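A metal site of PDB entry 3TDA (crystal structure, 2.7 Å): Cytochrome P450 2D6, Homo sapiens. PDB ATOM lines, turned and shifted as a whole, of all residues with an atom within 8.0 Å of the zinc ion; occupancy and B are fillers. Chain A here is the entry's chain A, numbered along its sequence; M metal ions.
Three residues have an atom within 4 Å of the zinc ion: His 236, Asp 248 and Glu 251.
OE1 of Glu 251 lies within hydrogen-bond range of N of Arg 247, 3.1 Å away. OG1 of Thr 239 sits at hydrogen-bond distance from O of His 236, at 3.4 Å. The side-chain carboxylate of Asp 248 is in hydrogen-bond range of the backbone NH of Thr 250 (3.3 Å).
The zinc ion is bound by OE2 of Glu 251, NE2 of His 236 and OD2 of Asp 248.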
ATOM      1  N   ALA A 165     -25.355  -8.747  15.732  1.00  0.00           N
ATOM      2  CA  ALA A 165     -25.805  -8.414  14.377  1.00  0.00           C
ATOM      3  C   ALA A 165     -24.689  -7.634  13.672  1.00  0.00           C
ATOM      4  O   ALA A 165     -24.405  -7.864  12.502  1.00  0.00           O
ATOM      5  CB  ALA A 165     -27.074  -7.576  14.437  1.00  0.00           C
ATOM      6  N   SER A 166     -24.061  -6.702  14.384  1.00  0.00           N
ATOM      7  CA  SER A 166     -22.973  -5.898  13.827  1.00  0.00           C
ATOM      8  C   SER A 166     -21.845  -6.781  13.317  1.00  0.00           C
ATOM      9  O   SER A 166     -21.301  -6.569  12.245  1.00  0.00           O
ATOM     10  CB  SER A 166     -22.401  -4.937  14.893  1.00  0.00           C
ATOM     11  OG  SER A 166     -21.242  -4.262  14.420  1.00  0.00           O
ATOM     12  N   LEU A 167     -21.497  -7.776  14.128  1.00  0.00           N
ATOM     13  CA  LEU A 167     -20.430  -8.730  13.841  1.00  0.00           C
ATOM     14  C   LEU A 167     -20.765  -9.679  12.699  1.00  0.00           C
ATOM     15  O   LEU A 167     -19.950  -9.917  11.814  1.00  0.00           O
ATOM     16  CB  LEU A 167     -20.128  -9.559  15.094  1.00  0.00           C
ATOM     17  CG  LEU A 167     -18.937  -9.306  16.015  1.00  0.00           C
ATOM     18  CD1 LEU A 167     -18.344  -7.937  15.844  1.00  0.00           C
ATOM     19  CD2 LEU A 167     -19.412  -9.544  17.441  1.00  0.00           C
ATOM     20  N   THR A 168     -21.974 -10.218  12.718  1.00  0.00           N
ATOM     21  CA  THR A 168     -22.415 -11.151  11.704  1.00  0.00           C
ATOM     22  C   THR A 168     -23.026 -10.506  10.476  1.00  0.00           C
ATOM     23  O   THR A 168     -22.623 -10.793   9.347  1.00  0.00           O
ATOM     24  CB  THR A 168     -23.442 -12.147  12.275  1.00  0.00           C
ATOM     25  OG1 THR A 168     -24.600 -11.440  12.738  1.00  0.00           O
ATOM     26  CG2 THR A 168     -22.847 -12.883  13.458  1.00  0.00           C
ATOM     27  N   CYS A 169     -23.983  -9.610  10.692  1.00  0.00           N
ATOM     28  CA  CYS A 169     -24.684  -8.924   9.603  1.00  0.00           C
ATOM     29  C   CYS A 169     -24.149  -7.547   9.240  1.00  0.00           C
ATOM     30  O   CYS A 169     -24.701  -6.899   8.369  1.00  0.00           O
ATOM     31  CB  CYS A 169     -26.166  -8.820   9.963  1.00  0.00           C
ATOM     32  SG  CYS A 169     -27.004 -10.410  10.174  1.00  0.00           S
ATOM     33  N   GLY A 170     -23.100  -7.078   9.896  1.00  0.00           N
ATOM     34  CA  GLY A 170     -22.555  -5.766   9.588  1.00  0.00           C
ATOM     35  C   GLY A 170     -23.460  -4.541   9.838  1.00  0.00           C
ATOM     36  O   GLY A 170     -23.217  -3.483   9.304  1.00  0.00           O
ATOM     37  N   ARG A 171     -24.490  -4.658  10.670  1.00  0.00           N
ATOM     38  CA  ARG A 171     -25.363  -3.522  10.891  1.00  0.00           C
ATOM     39  C   ARG A 171     -26.106  -3.657  12.200  1.00  0.00           C
ATOM     40  O   ARG A 171     -26.110  -4.717  12.808  1.00  0.00           O
ATOM     41  CB  ARG A 171     -26.407  -3.436   9.781  1.00  0.00           C
ATOM     42  CG  ARG A 171     -27.325  -4.674   9.745  1.00  0.00           C
ATOM     43  CD  ARG A 171     -28.550  -4.445   8.924  1.00  0.00           C
ATOM     44  NE  ARG A 171     -29.319  -3.313   9.452  1.00  0.00           N
ATOM     45  CZ  ARG A 171     -30.417  -2.809   8.897  1.00  0.00           C
ATOM     46  NH1 ARG A 171     -30.916  -3.328   7.788  1.00  0.00           N
ATOM     47  NH2 ARG A 171     -31.024  -1.791   9.470  1.00  0.00           N
ATOM     48  N   HIS A 236     -27.969  -8.295   2.160  1.00  0.00           N
ATOM     49  CA  HIS A 236     -26.532  -8.221   2.406  1.00  0.00           C
ATOM     50  C   HIS A 236     -25.727  -8.698   1.217  1.00  0.00           C
ATOM     51  O   HIS A 236     -24.692  -8.110   0.876  1.00  0.00           O
ATOM     52  CB  HIS A 236     -26.166  -9.039   3.651  1.00  0.00           C
ATOM     53  CG  HIS A 236     -24.860  -8.654   4.262  1.00  0.00           C
ATOM     54  ND1 HIS A 236     -24.475  -9.080   5.510  1.00  0.00           N
ATOM     55  CD2 HIS A 236     -23.861  -7.860   3.811  1.00  0.00           C
ATOM     56  CE1 HIS A 236     -23.294  -8.570   5.800  1.00  0.00           C
ATOM     57  NE2 HIS A 236     -22.898  -7.827   4.789  1.00  0.00           N
ATOM     58  N   ARG A 237     -26.187  -9.763   0.569  1.00  0.00           N
ATOM     59  CA  ARG A 237     -25.468 -10.278  -0.583  1.00  0.00           C
ATOM     60  C   ARG A 237     -25.430  -9.167  -1.622  1.00  0.00           C
ATOM     61  O   ARG A 237     -24.477  -9.069  -2.410  1.00  0.00           O
ATOM     62  CB  ARG A 237     -26.162 -11.526  -1.114  1.00  0.00           C
ATOM     63  CG  ARG A 237     -25.419 -12.247  -2.236  1.00  0.00           C
ATOM     64  CD  ARG A 237     -25.037 -13.694  -1.865  1.00  0.00           C
ATOM     65  NE  ARG A 237     -26.106 -14.425  -1.166  1.00  0.00           N
ATOM     66  CZ  ARG A 237     -26.024 -15.727  -0.859  1.00  0.00           C
ATOM     67  NH1 ARG A 237     -24.943 -16.422  -1.195  1.00  0.00           N
ATOM     68  NH2 ARG A 237     -27.029 -16.326  -0.218  1.00  0.00           N
ATOM     69  N   THR A 239     -25.514  -5.674  -0.937  1.00  0.00           N
ATOM     70  CA  THR A 239     -24.686  -4.532  -0.531  1.00  0.00           C
ATOM     71  C   THR A 239     -23.203  -4.882  -0.391  1.00  0.00           C
ATOM     72  O   THR A 239     -22.339  -4.017  -0.452  1.00  0.00           O
ATOM     73  CB  THR A 239     -25.192  -3.932   0.823  1.00  0.00           C
ATOM     74  OG1 THR A 239     -24.999  -4.892   1.879  1.00  0.00           O
ATOM     75  CG2 THR A 239     -26.684  -3.586   0.733  1.00  0.00           C
ATOM     76  N   TRP A 240     -22.909  -6.169  -0.222  1.00  0.00           N
ATOM     77  CA  TRP A 240     -21.536  -6.639  -0.060  1.00  0.00           C
ATOM     78  C   TRP A 240     -20.603  -6.135  -1.159  1.00  0.00           C
ATOM     79  O   TRP A 240     -20.941  -6.159  -2.345  1.00  0.00           O
ATOM     80  CB  TRP A 240     -21.523  -8.172  -0.011  1.00  0.00           C
ATOM     81  CG  TRP A 240     -20.177  -8.797  -0.011  1.00  0.00           C
ATOM     82  CD1 TRP A 240     -19.074  -8.384   0.707  1.00  0.00           C
ATOM     83  CD2 TRP A 240     -19.786  -9.997  -0.687  1.00  0.00           C
ATOM     84  NE1 TRP A 240     -18.021  -9.256   0.508  1.00  0.00           N
ATOM     85  CE2 TRP A 240     -18.430 -10.256  -0.336  1.00  0.00           C
ATOM     86  CE3 TRP A 240     -20.436 -10.880  -1.560  1.00  0.00           C
ATOM     87  CZ2 TRP A 240     -17.715 -11.363  -0.824  1.00  0.00           C
ATOM     88  CZ3 TRP A 240     -19.719 -11.997  -2.038  1.00  0.00           C
ATOM     89  CH2 TRP A 240     -18.387 -12.222  -1.666  1.00  0.00           C
ATOM     90  N   ASP A 241     -19.438  -5.654  -0.740  1.00  0.00           N
ATOM     91  CA  ASP A 241     -18.405  -5.163  -1.643  1.00  0.00           C
ATOM     92  C   ASP A 241     -17.223  -6.145  -1.527  1.00  0.00           C
ATOM     93  O   ASP A 241     -16.382  -6.020  -0.639  1.00  0.00           O
ATOM     94  CB  ASP A 241     -17.972  -3.757  -1.247  1.00  0.00           C
ATOM     95  CG  ASP A 241     -16.925  -3.169  -2.189  1.00  0.00           C
ATOM     96  OD1 ASP A 241     -16.544  -2.000  -1.969  1.00  0.00           O
ATOM     97  OD2 ASP A 241     -16.498  -3.868  -3.137  1.00  0.00           O
ATOM     98  N   PRO A 245     -11.875  -5.919   2.176  1.00  0.00           N
ATOM     99  CA  PRO A 245     -11.766  -7.011   3.142  1.00  0.00           C
ATOM    100  C   PRO A 245     -13.121  -7.129   3.858  1.00  0.00           C
ATOM    101  O   PRO A 245     -13.769  -6.110   4.114  1.00  0.00           O
ATOM    102  CB  PRO A 245     -10.656  -6.529   4.083  1.00  0.00           C
ATOM    103  CG  PRO A 245      -9.813  -5.641   3.185  1.00  0.00           C
ATOM    104  CD  PRO A 245     -10.853  -4.892   2.411  1.00  0.00           C
ATOM    105  N   PRO A 246     -13.550  -8.351   4.205  1.00  0.00           N
ATOM    106  CA  PRO A 246     -14.834  -8.531   4.879  1.00  0.00           C
ATOM    107  C   PRO A 246     -15.050  -7.631   6.096  1.00  0.00           C
ATOM    108  O   PRO A 246     -14.161  -7.487   6.919  1.00  0.00           O
ATOM    109  CB  PRO A 246     -14.822 -10.008   5.243  1.00  0.00           C
ATOM    110  CG  PRO A 246     -14.087 -10.610   4.111  1.00  0.00           C
ATOM    111  CD  PRO A 246     -12.916  -9.656   3.961  1.00  0.00           C
ATOM    112  N   ARG A 247     -16.221  -7.017   6.199  1.00  0.00           N
ATOM    113  CA  ARG A 247     -16.556  -6.150   7.323  1.00  0.00           C
ATOM    114  C   ARG A 247     -17.239  -6.956   8.425  1.00  0.00           C
ATOM    115  O   ARG A 247     -17.323  -6.525   9.569  1.00  0.00           O
ATOM    116  CB  ARG A 247     -17.562  -5.078   6.921  1.00  0.00           C
ATOM    117  CG  ARG A 247     -17.225  -4.199   5.765  1.00  0.00           C
ATOM    118  CD  ARG A 247     -17.899  -2.838   5.975  1.00  0.00           C
ATOM    119  NE  ARG A 247     -19.236  -3.028   6.531  1.00  0.00           N
ATOM    120  CZ  ARG A 247     -19.623  -2.647   7.751  1.00  0.00           C
ATOM    121  NH1 ARG A 247     -18.784  -2.051   8.565  1.00  0.00           N
ATOM    122  NH2 ARG A 247     -20.864  -2.911   8.152  1.00  0.00           N
ATOM    123  N   ASP A 248     -17.783  -8.105   8.065  1.00  0.00           N
ATOM    124  CA  ASP A 248     -18.513  -8.903   9.033  1.00  0.00           C
ATOM    125  C   ASP A 248     -18.336 -10.370   8.721  1.00  0.00           C
ATOM    126  O   ASP A 248     -17.702 -10.713   7.738  1.00  0.00           O
ATOM    127  CB  ASP A 248     -19.980  -8.510   8.983  1.00  0.00           C
ATOM    128  CG  ASP A 248     -20.495  -8.381   7.561  1.00  0.00           C
ATOM    129  OD1 ASP A 248     -20.672  -9.410   6.870  1.00  0.00           O
ATOM    130  OD2 ASP A 248     -20.704  -7.233   7.123  1.00  0.00           O
ATOM    131  N   LEU A 249     -18.915 -11.211   9.571  1.00  0.00           N
ATOM    132  CA  LEU A 249     -18.803 -12.656   9.404  1.00  0.00           C
ATOM    133  C   LEU A 249     -19.561 -13.164   8.171  1.00  0.00           C
ATOM    134  O   LEU A 249     -19.138 -14.124   7.546  1.00  0.00           O
ATOM    135  CB  LEU A 249     -19.288 -13.377  10.658  1.00  0.00           C
ATOM    136  CG  LEU A 249     -19.051 -14.892  10.672  1.00  0.00           C
ATOM    137  CD1 LEU A 249     -18.569 -15.326  12.040  1.00  0.00           C
ATOM    138  CD2 LEU A 249     -20.320 -15.637  10.301  1.00  0.00           C
ATOM    139  N   THR A 250     -20.681 -12.538   7.840  1.00  0.00           N
ATOM    140  CA  THR A 250     -21.421 -12.967   6.664  1.00  0.00           C
ATOM    141  C   THR A 250     -20.572 -12.736   5.402  1.00  0.00           C
ATOM    142  O   THR A 250     -20.560 -13.559   4.486  1.00  0.00           O
ATOM    143  CB  THR A 250     -22.761 -12.204   6.575  1.00  0.00           C
ATOM    144  OG1 THR A 250     -23.630 -12.650   7.622  1.00  0.00           O
ATOM    145  CG2 THR A 250     -23.435 -12.429   5.228  1.00  0.00           C
ATOM    146  N   GLU A 251     -19.854 -11.617   5.342  1.00  0.00           N
ATOM    147  CA  GLU A 251     -19.033 -11.354   4.164  1.00  0.00           C
ATOM    148  C   GLU A 251     -17.873 -12.346   4.151  1.00  0.00           C
ATOM    149  O   GLU A 251     -17.587 -12.944   3.109  1.00  0.00           O
ATOM    150  CB  GLU A 251     -18.502  -9.922   4.146  1.00  0.00           C
ATOM    151  CG  GLU A 251     -19.537  -8.898   3.713  1.00  0.00           C
ATOM    152  CD  GLU A 251     -19.056  -7.454   3.907  1.00  0.00           C
ATOM    153  OE1 GLU A 251     -17.865  -7.173   3.600  1.00  0.00           O
ATOM    154  OE2 GLU A 251     -19.863  -6.594   4.365  1.00  0.00           O
ATOM    155  N   ALA A 252     -17.235 -12.537   5.300  1.00  0.00           N
ATOM    156  CA  ALA A 252     -16.125 -13.476   5.356  1.00  0.00           C
ATOM    157  C   ALA A 252     -16.626 -14.827   4.850  1.00  0.00           C
ATOM    158  O   ALA A 252     -15.969 -15.447   4.000  1.00  0.00           O
ATOM    159  CB  ALA A 252     -15.606 -13.603   6.769  1.00  0.00           C
ATOM    160  N   LEU A 254     -19.178 -15.495   2.892  1.00  0.00           N
ATOM    161  CA  LEU A 254     -19.425 -15.351   1.460  1.00  0.00           C
ATOM    162  C   LEU A 254     -18.139 -15.504   0.651  1.00  0.00           C
ATOM    163  O   LEU A 254     -18.102 -16.260  -0.307  1.00  0.00           O
ATOM    164  CB  LEU A 254     -20.061 -13.993   1.130  1.00  0.00           C
ATOM    165  CG  LEU A 254     -21.502 -13.751   1.600  1.00  0.00           C
ATOM    166  CD1 LEU A 254     -21.885 -12.309   1.367  1.00  0.00           C
ATOM    167  CD2 LEU A 254     -22.455 -14.691   0.889  1.00  0.00           C
HETATM  168 ZN    ZN M   1     -21.416  -6.625   5.277  1.00  0.00          ZN
